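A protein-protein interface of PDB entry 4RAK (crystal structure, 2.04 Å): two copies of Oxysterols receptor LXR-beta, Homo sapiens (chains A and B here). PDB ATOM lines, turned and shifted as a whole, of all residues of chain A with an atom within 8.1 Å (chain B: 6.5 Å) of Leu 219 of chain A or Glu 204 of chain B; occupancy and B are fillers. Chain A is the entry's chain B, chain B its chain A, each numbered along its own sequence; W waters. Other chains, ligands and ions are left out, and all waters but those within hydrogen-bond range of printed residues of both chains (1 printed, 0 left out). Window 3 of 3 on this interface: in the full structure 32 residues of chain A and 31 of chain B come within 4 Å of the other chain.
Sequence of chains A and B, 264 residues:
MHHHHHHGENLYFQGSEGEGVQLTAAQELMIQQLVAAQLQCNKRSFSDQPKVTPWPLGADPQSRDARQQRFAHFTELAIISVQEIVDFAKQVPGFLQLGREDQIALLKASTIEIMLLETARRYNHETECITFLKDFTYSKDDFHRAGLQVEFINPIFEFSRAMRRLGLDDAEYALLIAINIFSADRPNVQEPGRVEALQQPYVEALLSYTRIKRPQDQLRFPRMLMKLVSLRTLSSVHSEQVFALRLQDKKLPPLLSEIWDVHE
Of the 15 printed residues of chain A, 4 touch a printed residue of chain B.
Hydrophobic or aromatic side chains of chain A that line the printed part of chain B: Leu 219 and Pro 222.
Along chain A the printed residues that touch a printed residue of chain B span positions 218 to 223.
Printed residues of chain B that touch a printed residue of chain A: Gln 200, Val 203, Glu 204, Leu 207 and Phe 221.
Hydrophobic or aromatic side chains of chain B that line the printed part of chain A: Val 203, Leu 207 and Phe 221.
Along chain B the printed residues that touch a printed residue of chain A span positions 200 to 221.
Among the printed residues, no Asp or Glu carboxylate lies within 4 Å of a Lys or Arg side-chain nitrogen of the other chain.
The backbone carbonyl oxygen (O) of Glu 204 of chain B is in hydrogen-bond range of the side-chain hydroxyl (OG) of Ser 208 of chain B, 3.1 Å away.
The side-chain carboxylate (OD1) of Asp 217 of chain A lies close to the backbone NH (N) of Leu 219 of chain A (3.4 Å).
The guanidinium group of Arg 223 of chain A lies within salt-bridge range of the side-chain carboxylate of Asp 217 of chain A, at 3.1 Å.
Water W1 bridges OE1 of Gln 200 of chain B and O of Leu 219 of chain A.
1 position is printed for both chains.
Of the 7 pairs that touch across the chains among the printed residues, none has its exchanged pair printed and touching as well.
Leu 219 of chain A touches three residues of chain B.
Of the printed residues of chain A, Leu 207 of chain B touches Gln 218 (3.9 Å).
Of the printed residues of chain A, Phe 221 of chain B touches Pro 222.
Of the printed residues of chain B, Pro 222 of chain A touches Val 203 (3.6 Å) and Phe 221 (3.6 Å).
Of the printed residues of chain A, Gln 200 of chain B touches Leu 219 and Arg 223.
Of the printed residues of chain B, Gln 218 of chain A touches Leu 207.
Leu 166 of chain A touches none of the printed residues of chain B.
The nearest residue of chain B that does not touch Leu 219 of chain A is Leu 207 of chain B (4.8 Å).
The side-chain amide oxygen (OE1) of Gln 200 of chain B is in hydrogen-bond range of the guanidinium group (NH1) of Arg 223 of chain A (3.4 Å).
Among the printed residues, merely in contact across the chains: Gln 218 of chain A with Leu 207 of chain B (3.9 Å), Leu 219 of chain A with Gln 200 of chain B (3.9 Å), Leu 219 of chain A with Val 203 of chain B (3.9 Å), Leu 219 of chain A with Glu 204 of chain B (3.6 Å), Pro 222 of chain A with Val 203 of chain B (3.6 Å) and Pro 222 of chain A with Phe 221 of chain B (3.6 Å).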
ATOM      1  N   LEU A 166      11.194  23.245 -17.021  1.00  0.00           N
ATOM      2  CA  LEU A 166      10.213  22.319 -17.597  1.00  0.00           C
ATOM      3  C   LEU A 166       9.633  21.378 -16.540  1.00  0.00           C
ATOM      4  O   LEU A 166       8.587  20.759 -16.745  1.00  0.00           O
ATOM      5  CB  LEU A 166      10.876  21.555 -18.741  1.00  0.00           C
ATOM      6  CG  LEU A 166      10.575  21.938 -20.182  1.00  0.00           C
ATOM      7  CD1 LEU A 166      10.150  23.372 -20.318  1.00  0.00           C
ATOM      8  CD2 LEU A 166      11.745  21.588 -21.096  1.00  0.00           C
ATOM      9  N   THR A 210       2.641  13.321 -20.803  1.00  0.00           N
ATOM     10  CA  THR A 210       2.632  14.781 -20.641  1.00  0.00           C
ATOM     11  C   THR A 210       1.203  15.339 -20.589  1.00  0.00           C
ATOM     12  O   THR A 210       0.944  16.243 -19.791  1.00  0.00           O
ATOM     13  CB  THR A 210       3.498  15.481 -21.718  1.00  0.00           C
ATOM     14  OG1 THR A 210       3.147  14.989 -23.007  1.00  0.00           O
ATOM     15  CG2 THR A 210       4.979  15.251 -21.495  1.00  0.00           C
ATOM     16  N   ARG A 214       0.095  17.557 -17.144  1.00  0.00           N
ATOM     17  CA  ARG A 214      -0.288  18.966 -17.271  1.00  0.00           C
ATOM     18  C   ARG A 214      -1.358  19.063 -18.379  1.00  0.00           C
ATOM     19  O   ARG A 214      -1.033  19.388 -19.529  1.00  0.00           O
ATOM     20  CB  ARG A 214       0.918  19.880 -17.586  1.00  0.00           C
ATOM     21  CG  ARG A 214       2.056  19.886 -16.566  1.00  0.00           C
ATOM     22  CD  ARG A 214       1.835  20.846 -15.409  1.00  0.00           C
ATOM     23  NE  ARG A 214       2.771  20.572 -14.311  1.00  0.00           N
ATOM     24  CZ  ARG A 214       2.515  19.782 -13.268  1.00  0.00           C
ATOM     25  NH1 ARG A 214       1.336  19.183 -13.143  1.00  0.00           N
ATOM     26  NH2 ARG A 214       3.439  19.588 -12.336  1.00  0.00           N
ATOM     27  N   PRO A 215      -2.640  18.772 -18.060  1.00  0.00           N
ATOM     28  CA  PRO A 215      -3.660  18.790 -19.119  1.00  0.00           C
ATOM     29  C   PRO A 215      -3.881  20.159 -19.735  1.00  0.00           C
ATOM     30  O   PRO A 215      -4.259  20.226 -20.898  1.00  0.00           O
ATOM     31  CB  PRO A 215      -4.921  18.242 -18.419  1.00  0.00           C
ATOM     32  CG  PRO A 215      -4.432  17.584 -17.181  1.00  0.00           C
ATOM     33  CD  PRO A 215      -3.224  18.364 -16.764  1.00  0.00           C
ATOM     34  N   GLN A 216      -3.601  21.237 -18.981  1.00  0.00           N
ATOM     35  CA  GLN A 216      -3.820  22.584 -19.490  1.00  0.00           C
ATOM     36  C   GLN A 216      -2.581  23.196 -20.186  1.00  0.00           C
ATOM     37  O   GLN A 216      -2.767  24.168 -20.905  1.00  0.00           O
ATOM     38  CB  GLN A 216      -4.368  23.545 -18.399  1.00  0.00           C
ATOM     39  CG  GLN A 216      -5.532  23.009 -17.540  1.00  0.00           C
ATOM     40  CD  GLN A 216      -6.668  22.373 -18.327  1.00  0.00           C
ATOM     41  OE1 GLN A 216      -7.193  22.941 -19.292  1.00  0.00           O
ATOM     42  NE2 GLN A 216      -7.078  21.180 -17.908  1.00  0.00           N
ATOM     43  N   ASP A 217      -1.345  22.651 -20.006  1.00  0.00           N
ATOM     44  CA  ASP A 217      -0.198  23.255 -20.707  1.00  0.00           C
ATOM     45  C   ASP A 217      -0.246  22.947 -22.202  1.00  0.00           C
ATOM     46  O   ASP A 217      -0.611  23.827 -22.979  1.00  0.00           O
ATOM     47  CB  ASP A 217       1.161  22.935 -20.093  1.00  0.00           C
ATOM     48  CG  ASP A 217       2.245  23.971 -20.456  1.00  0.00           C
ATOM     49  OD1 ASP A 217       2.217  24.504 -21.595  1.00  0.00           O
ATOM     50  OD2 ASP A 217       3.084  24.287 -19.588  1.00  0.00           O
ATOM     51  N   GLN A 218       0.102  21.733 -22.610  1.00  0.00           N
ATOM     52  CA  GLN A 218       0.081  21.270 -24.021  1.00  0.00           C
ATOM     53  C   GLN A 218       1.284  21.718 -24.845  1.00  0.00           C
ATOM     54  O   GLN A 218       1.647  21.035 -25.779  1.00  0.00           O
ATOM     55  CB  GLN A 218      -1.230  21.564 -24.765  1.00  0.00           C
ATOM     56  CG  GLN A 218      -2.117  20.328 -24.920  1.00  0.00           C
ATOM     57  CD  GLN A 218      -3.408  20.623 -25.645  1.00  0.00           C
ATOM     58  OE1 GLN A 218      -4.444  20.874 -25.027  1.00  0.00           O
ATOM     59  NE2 GLN A 218      -3.367  20.597 -26.971  1.00  0.00           N
ATOM     60  N   LEU A 219       1.907  22.839 -24.490  1.00  0.00           N
ATOM     61  CA  LEU A 219       3.120  23.284 -25.150  1.00  0.00           C
ATOM     62  C   LEU A 219       4.349  22.665 -24.483  1.00  0.00           C
ATOM     63  O   LEU A 219       5.459  22.783 -24.997  1.00  0.00           O
ATOM     64  CB  LEU A 219       3.202  24.823 -25.133  1.00  0.00           C
ATOM     65  CG  LEU A 219       2.276  25.547 -26.110  1.00  0.00           C
ATOM     66  CD1 LEU A 219       2.349  27.050 -25.893  1.00  0.00           C
ATOM     67  CD2 LEU A 219       2.638  25.203 -27.552  1.00  0.00           C
ATOM     68  N   ARG A 220       4.146  22.002 -23.339  1.00  0.00           N
ATOM     69  CA  ARG A 220       5.221  21.385 -22.554  1.00  0.00           C
ATOM     70  C   ARG A 220       5.918  20.232 -23.303  1.00  0.00           C
ATOM     71  O   ARG A 220       7.150  20.168 -23.310  1.00  0.00           O
ATOM     72  CB  ARG A 220       4.693  20.941 -21.195  1.00  0.00           C
ATOM     73  CG  ARG A 220       5.745  21.006 -20.086  1.00  0.00           C
ATOM     74  CD  ARG A 220       5.157  20.717 -18.728  1.00  0.00           C
ATOM     75  NE  ARG A 220       6.099  19.997 -17.880  1.00  0.00           N
ATOM     76  CZ  ARG A 220       6.154  18.674 -17.773  1.00  0.00           C
ATOM     77  NH1 ARG A 220       5.339  17.913 -18.474  1.00  0.00           N
ATOM     78  NH2 ARG A 220       7.035  18.110 -16.981  1.00  0.00           N
ATOM     79  N   PHE A 221       5.126  19.356 -23.932  1.00  0.00           N
ATOM     80  CA  PHE A 221       5.585  18.221 -24.722  1.00  0.00           C
ATOM     81  C   PHE A 221       6.464  18.700 -25.886  1.00  0.00           C
ATOM     82  O   PHE A 221       7.646  18.353 -25.882  1.00  0.00           O
ATOM     83  CB  PHE A 221       4.432  17.312 -25.147  1.00  0.00           C
ATOM     84  CG  PHE A 221       4.793  16.220 -26.129  1.00  0.00           C
ATOM     85  CD1 PHE A 221       5.631  15.180 -25.765  1.00  0.00           C
ATOM     86  CD2 PHE A 221       4.274  16.220 -27.413  1.00  0.00           C
ATOM     87  CE1 PHE A 221       5.954  14.182 -26.669  1.00  0.00           C
ATOM     88  CE2 PHE A 221       4.622  15.230 -28.330  1.00  0.00           C
ATOM     89  CZ  PHE A 221       5.441  14.196 -27.937  1.00  0.00           C
ATOM     90  N   PRO A 222       5.983  19.601 -26.794  1.00  0.00           N
ATOM     91  CA  PRO A 222       6.894  20.118 -27.848  1.00  0.00           C
ATOM     92  C   PRO A 222       8.120  20.791 -27.290  1.00  0.00           C
ATOM     93  O   PRO A 222       9.184  20.699 -27.895  1.00  0.00           O
ATOM     94  CB  PRO A 222       6.031  21.120 -28.612  1.00  0.00           C
ATOM     95  CG  PRO A 222       4.631  20.721 -28.345  1.00  0.00           C
ATOM     96  CD  PRO A 222       4.610  20.124 -26.968  1.00  0.00           C
ATOM     97  N   ARG A 223       7.993  21.464 -26.130  1.00  0.00           N
ATOM     98  CA  ARG A 223       9.140  22.139 -25.495  1.00  0.00           C
ATOM     99  C   ARG A 223      10.213  21.121 -25.116  1.00  0.00           C
ATOM    100  O   ARG A 223      11.423  21.428 -25.175  1.00  0.00           O
ATOM    101  CB  ARG A 223       8.702  22.974 -24.263  1.00  0.00           C
ATOM    102  CG  ARG A 223       8.358  24.428 -24.550  1.00  0.00           C
ATOM    103  CD  ARG A 223       8.418  25.328 -23.315  1.00  0.00           C
ATOM    104  NE  ARG A 223       7.285  25.092 -22.433  1.00  0.00           N
ATOM    105  CZ  ARG A 223       6.152  25.798 -22.422  1.00  0.00           C
ATOM    106  NH1 ARG A 223       6.002  26.849 -23.226  1.00  0.00           N
ATOM    107  NH2 ARG A 223       5.164  25.465 -21.586  1.00  0.00           N
ATOM    108  N   MET A 224       9.780  19.897 -24.746  1.00  0.00           N
ATOM    109  CA  MET A 224      10.684  18.780 -24.386  1.00  0.00           C
ATOM    110  C   MET A 224      11.419  18.264 -25.572  1.00  0.00           C
ATOM    111  O   MET A 224      12.628  18.106 -25.525  1.00  0.00           O
ATOM    112  CB  MET A 224       9.925  17.629 -23.717  1.00  0.00           C
ATOM    113  CG  MET A 224       9.655  17.865 -22.272  1.00  0.00           C
ATOM    114  SD  MET A 224       8.826  16.413 -21.607  1.00  0.00           S
ATOM    115  CE  MET A 224       7.859  17.228 -20.447  1.00  0.00           C
ATOM    116  N   LEU A 225      10.693  18.030 -26.651  1.00  0.00           N
ATOM    117  CA  LEU A 225      11.227  17.503 -27.904  1.00  0.00           C
ATOM    118  C   LEU A 225      12.232  18.493 -28.496  1.00  0.00           C
ATOM    119  O   LEU A 225      13.208  18.081 -29.111  1.00  0.00           O
ATOM    120  CB  LEU A 225      10.080  17.319 -28.864  1.00  0.00           C
ATOM    121  CG  LEU A 225       9.541  15.940 -29.193  1.00  0.00           C
ATOM    122  CD1 LEU A 225       9.785  14.922 -28.083  1.00  0.00           C
ATOM    123  CD2 LEU A 225       8.094  16.036 -29.655  1.00  0.00           C
ATOM    124  N   MET A 226      11.995  19.810 -28.284  1.00  0.00           N
ATOM    125  CA  MET A 226      12.879  20.870 -28.764  1.00  0.00           C
ATOM    126  C   MET A 226      14.222  20.863 -28.066  1.00  0.00           C
ATOM    127  O   MET A 226      15.210  21.326 -28.628  1.00  0.00           O
ATOM    128  CB  MET A 226      12.203  22.238 -28.666  1.00  0.00           C
ATOM    129  CG  MET A 226      12.312  23.024 -29.949  1.00  0.00           C
ATOM    130  SD  MET A 226      11.004  22.694 -31.146  1.00  0.00           S
ATOM    131  CE  MET A 226      11.649  21.332 -32.027  1.00  0.00           C
ATOM    132  N   GLN B  27      -4.897  32.319 -35.332  1.00  0.00           N
ATOM    133  CA  GLN B  27      -4.130  31.274 -35.967  1.00  0.00           C
ATOM    134  C   GLN B  27      -4.336  31.270 -37.463  1.00  0.00           C
ATOM    135  O   GLN B  27      -3.360  31.236 -38.206  1.00  0.00           O
ATOM    136  CB  GLN B  27      -4.476  29.908 -35.377  1.00  0.00           C
ATOM    137  CG  GLN B  27      -3.929  29.711 -33.955  1.00  0.00           C
ATOM    138  CD  GLN B  27      -4.326  28.391 -33.318  1.00  0.00           C
ATOM    139  OE1 GLN B  27      -3.629  27.864 -32.458  1.00  0.00           O
ATOM    140  NE2 GLN B  27      -5.454  27.847 -33.706  1.00  0.00           N
ATOM    141  N   ILE B 179       9.346  28.557 -36.529  1.00  0.00           N
ATOM    142  CA  ILE B 179       9.797  27.855 -35.333  1.00  0.00           C
ATOM    143  C   ILE B 179      11.340  27.796 -35.363  1.00  0.00           C
ATOM    144  O   ILE B 179      11.980  28.030 -34.348  1.00  0.00           O
ATOM    145  CB  ILE B 179       9.187  26.428 -35.180  1.00  0.00           C
ATOM    146  CG1 ILE B 179       7.655  26.478 -34.939  1.00  0.00           C
ATOM    147  CG2 ILE B 179       9.870  25.663 -34.044  1.00  0.00           C
ATOM    148  CD1 ILE B 179       6.875  25.167 -35.205  1.00  0.00           C
ATOM    149  N   GLN B 199       8.662  32.018 -30.154  1.00  0.00           N
ATOM    150  CA  GLN B 199       8.553  30.736 -30.859  1.00  0.00           C
ATOM    151  C   GLN B 199       7.209  30.036 -30.565  1.00  0.00           C
ATOM    152  O   GLN B 199       6.687  29.367 -31.417  1.00  0.00           O
ATOM    153  CB  GLN B 199       9.680  29.795 -30.410  1.00  0.00           C
ATOM    154  CG  GLN B 199       9.793  28.543 -31.298  1.00  0.00           C
ATOM    155  CD  GLN B 199      10.897  27.618 -30.837  1.00  0.00           C
ATOM    156  OE1 GLN B 199      11.026  27.304 -29.676  1.00  0.00           O
ATOM    157  NE2 GLN B 199      11.727  27.193 -31.731  1.00  0.00           N
ATOM    158  N   GLN B 200       6.679  30.206 -29.347  1.00  0.00           N
ATOM    159  CA  GLN B 200       5.459  29.535 -28.876  1.00  0.00           C
ATOM    160  C   GLN B 200       4.220  29.669 -29.746  1.00  0.00           C
ATOM    161  O   GLN B 200       3.580  28.654 -29.942  1.00  0.00           O
ATOM    162  CB  GLN B 200       5.117  29.884 -27.423  1.00  0.00           C
ATOM    163  CG  GLN B 200       6.238  29.693 -26.450  1.00  0.00           C
ATOM    164  CD  GLN B 200       6.885  28.327 -26.543  1.00  0.00           C
ATOM    165  OE1 GLN B 200       6.216  27.299 -26.603  1.00  0.00           O
ATOM    166  NE2 GLN B 200       8.191  28.312 -26.609  1.00  0.00           N
ATOM    167  N   PRO B 201       3.822  30.854 -30.264  1.00  0.00           N
ATOM    168  CA  PRO B 201       2.586  30.900 -31.115  1.00  0.00           C
ATOM    169  C   PRO B 201       2.676  30.068 -32.390  1.00  0.00           C
ATOM    170  O   PRO B 201       1.651  29.678 -32.940  1.00  0.00           O
ATOM    171  CB  PRO B 201       2.484  32.369 -31.501  1.00  0.00           C
ATOM    172  CG  PRO B 201       3.321  33.093 -30.548  1.00  0.00           C
ATOM    173  CD  PRO B 201       4.428  32.184 -30.163  1.00  0.00           C
ATOM    174  N   TYR B 202       3.899  29.863 -32.894  1.00  0.00           N
ATOM    175  CA  TYR B 202       4.148  29.083 -34.117  1.00  0.00           C
ATOM    176  C   TYR B 202       4.098  27.593 -33.790  1.00  0.00           C
ATOM    177  O   TYR B 202       3.525  26.817 -34.561  1.00  0.00           O
ATOM    178  CB  TYR B 202       5.460  29.544 -34.808  1.00  0.00           C
ATOM    179  CG  TYR B 202       5.417  31.010 -35.102  1.00  0.00           C
ATOM    180  CD1 TYR B 202       4.680  31.502 -36.157  1.00  0.00           C
ATOM    181  CD2 TYR B 202       6.036  31.940 -34.243  1.00  0.00           C
ATOM    182  CE1 TYR B 202       4.558  32.879 -36.378  1.00  0.00           C
ATOM    183  CE2 TYR B 202       5.934  33.299 -34.476  1.00  0.00           C
ATOM    184  CZ  TYR B 202       5.163  33.763 -35.528  1.00  0.00           C
ATOM    185  OH  TYR B 202       5.044  35.105 -35.776  1.00  0.00           O
ATOM    186  N   VAL B 203       4.607  27.204 -32.606  1.00  0.00           N
ATOM    187  CA  VAL B 203       4.495  25.820 -32.103  1.00  0.00           C
ATOM    188  C   VAL B 203       2.970  25.494 -31.887  1.00  0.00           C
ATOM    189  O   VAL B 203       2.484  24.452 -32.356  1.00  0.00           O
ATOM    190  CB  VAL B 203       5.326  25.603 -30.818  1.00  0.00           C
ATOM    191  CG1 VAL B 203       5.167  24.191 -30.273  1.00  0.00           C
ATOM    192  CG2 VAL B 203       6.810  25.930 -31.042  1.00  0.00           C
ATOM    193  N   GLU B 204       2.215  26.427 -31.267  1.00  0.00           N
ATOM    194  CA  GLU B 204       0.765  26.320 -31.039  1.00  0.00           C
ATOM    195  C   GLU B 204      -0.006  26.165 -32.311  1.00  0.00           C
ATOM    196  O   GLU B 204      -0.886  25.286 -32.418  1.00  0.00           O
ATOM    197  CB  GLU B 204       0.219  27.609 -30.386  1.00  0.00           C
ATOM    198  CG  GLU B 204       0.266  27.688 -28.889  1.00  0.00           C
ATOM    199  CD  GLU B 204      -0.332  28.959 -28.304  1.00  0.00           C
ATOM    200  OE1 GLU B 204      -0.501  28.979 -27.065  1.00  0.00           O
ATOM    201  OE2 GLU B 204      -0.588  29.941 -29.056  1.00  0.00           O
ATOM    202  N   ALA B 205       0.293  27.045 -33.268  1.00  0.00           N
ATOM    203  CA  ALA B 205      -0.390  27.056 -34.544  1.00  0.00           C
ATOM    204  C   ALA B 205      -0.098  25.771 -35.318  1.00  0.00           C
ATOM    205  O   ALA B 205      -1.012  25.208 -35.899  1.00  0.00           O
ATOM    206  CB  ALA B 205      -0.019  28.281 -35.343  1.00  0.00           C
ATOM    207  N   LEU B 206       1.146  25.265 -35.258  1.00  0.00           N
ATOM    208  CA  LEU B 206       1.476  23.989 -35.927  1.00  0.00           C
ATOM    209  C   LEU B 206       0.736  22.777 -35.298  1.00  0.00           C
ATOM    210  O   LEU B 206       0.249  21.940 -36.005  1.00  0.00           O
ATOM    211  CB  LEU B 206       2.984  23.750 -36.013  1.00  0.00           C
ATOM    212  CG  LEU B 206       3.430  22.512 -36.799  1.00  0.00           C
ATOM    213  CD1 LEU B 206       3.092  22.654 -38.308  1.00  0.00           C
ATOM    214  CD2 LEU B 206       4.931  22.310 -36.663  1.00  0.00           C
ATOM    215  N   LEU B 207       0.637  22.737 -33.982  1.00  0.00           N
ATOM    216  CA  LEU B 207      -0.071  21.715 -33.229  1.00  0.00           C
ATOM    217  C   LEU B 207      -1.548  21.687 -33.646  1.00  0.00           C
ATOM    218  O   LEU B 207      -2.079  20.623 -33.911  1.00  0.00           O
ATOM    219  CB  LEU B 207       0.009  22.020 -31.733  1.00  0.00           C
ATOM    220  CG  LEU B 207       0.113  20.885 -30.739  1.00  0.00           C
ATOM    221  CD1 LEU B 207       0.178  21.427 -29.321  1.00  0.00           C
ATOM    222  CD2 LEU B 207      -1.059  19.930 -30.841  1.00  0.00           C
ATOM    223  N   SER B 208      -2.196  22.861 -33.712  1.00  0.00           N
ATOM    224  CA  SER B 208      -3.607  22.934 -34.112  1.00  0.00           C
ATOM    225  C   SER B 208      -3.812  22.554 -35.579  1.00  0.00           C
ATOM    226  O   SER B 208      -4.773  21.888 -35.906  1.00  0.00           O
ATOM    227  CB  SER B 208      -4.183  24.332 -33.833  1.00  0.00           C
ATOM    228  OG  SER B 208      -3.959  24.740 -32.510  1.00  0.00           O
ATOM    229  N   TYR B 209      -2.928  23.005 -36.459  1.00  0.00           N
ATOM    230  CA  TYR B 209      -3.050  22.745 -37.900  1.00  0.00           C
ATOM    231  C   TYR B 209      -2.883  21.254 -38.183  1.00  0.00           C
ATOM    232  O   TYR B 209      -3.632  20.712 -38.977  1.00  0.00           O
ATOM    233  CB  TYR B 209      -2.051  23.557 -38.703  1.00  0.00           C
ATOM    234  CG  TYR B 209      -2.273  23.552 -40.179  1.00  0.00           C
ATOM    235  CD1 TYR B 209      -1.697  22.574 -40.990  1.00  0.00           C
ATOM    236  CD2 TYR B 209      -2.999  24.564 -40.800  1.00  0.00           C
ATOM    237  CE1 TYR B 209      -1.848  22.602 -42.362  1.00  0.00           C
ATOM    238  CE2 TYR B 209      -3.172  24.582 -42.179  1.00  0.00           C
ATOM    239  CZ  TYR B 209      -2.609  23.594 -42.953  1.00  0.00           C
ATOM    240  OH  TYR B 209      -2.756  23.619 -44.310  1.00  0.00           O
ATOM    241  N   PHE B 221       2.808  15.459 -36.018  1.00  0.00           N
ATOM    242  CA  PHE B 221       3.325  16.671 -35.418  1.00  0.00           C
ATOM    243  C   PHE B 221       4.711  16.423 -34.745  1.00  0.00           C
ATOM    244  O   PHE B 221       5.677  16.986 -35.225  1.00  0.00           O
ATOM    245  CB  PHE B 221       2.276  17.341 -34.484  1.00  0.00           C
ATOM    246  CG  PHE B 221       2.809  18.490 -33.662  1.00  0.00           C
ATOM    247  CD1 PHE B 221       3.183  19.681 -34.261  1.00  0.00           C
ATOM    248  CD2 PHE B 221       2.975  18.365 -32.310  1.00  0.00           C
ATOM    249  CE1 PHE B 221       3.700  20.732 -33.505  1.00  0.00           C
ATOM    250  CE2 PHE B 221       3.500  19.414 -31.557  1.00  0.00           C
ATOM    251  CZ  PHE B 221       3.833  20.601 -32.167  1.00  0.00           C
HETATM  252  O   HOH W   1       6.412  24.729 -27.350  1.00  0.00           O
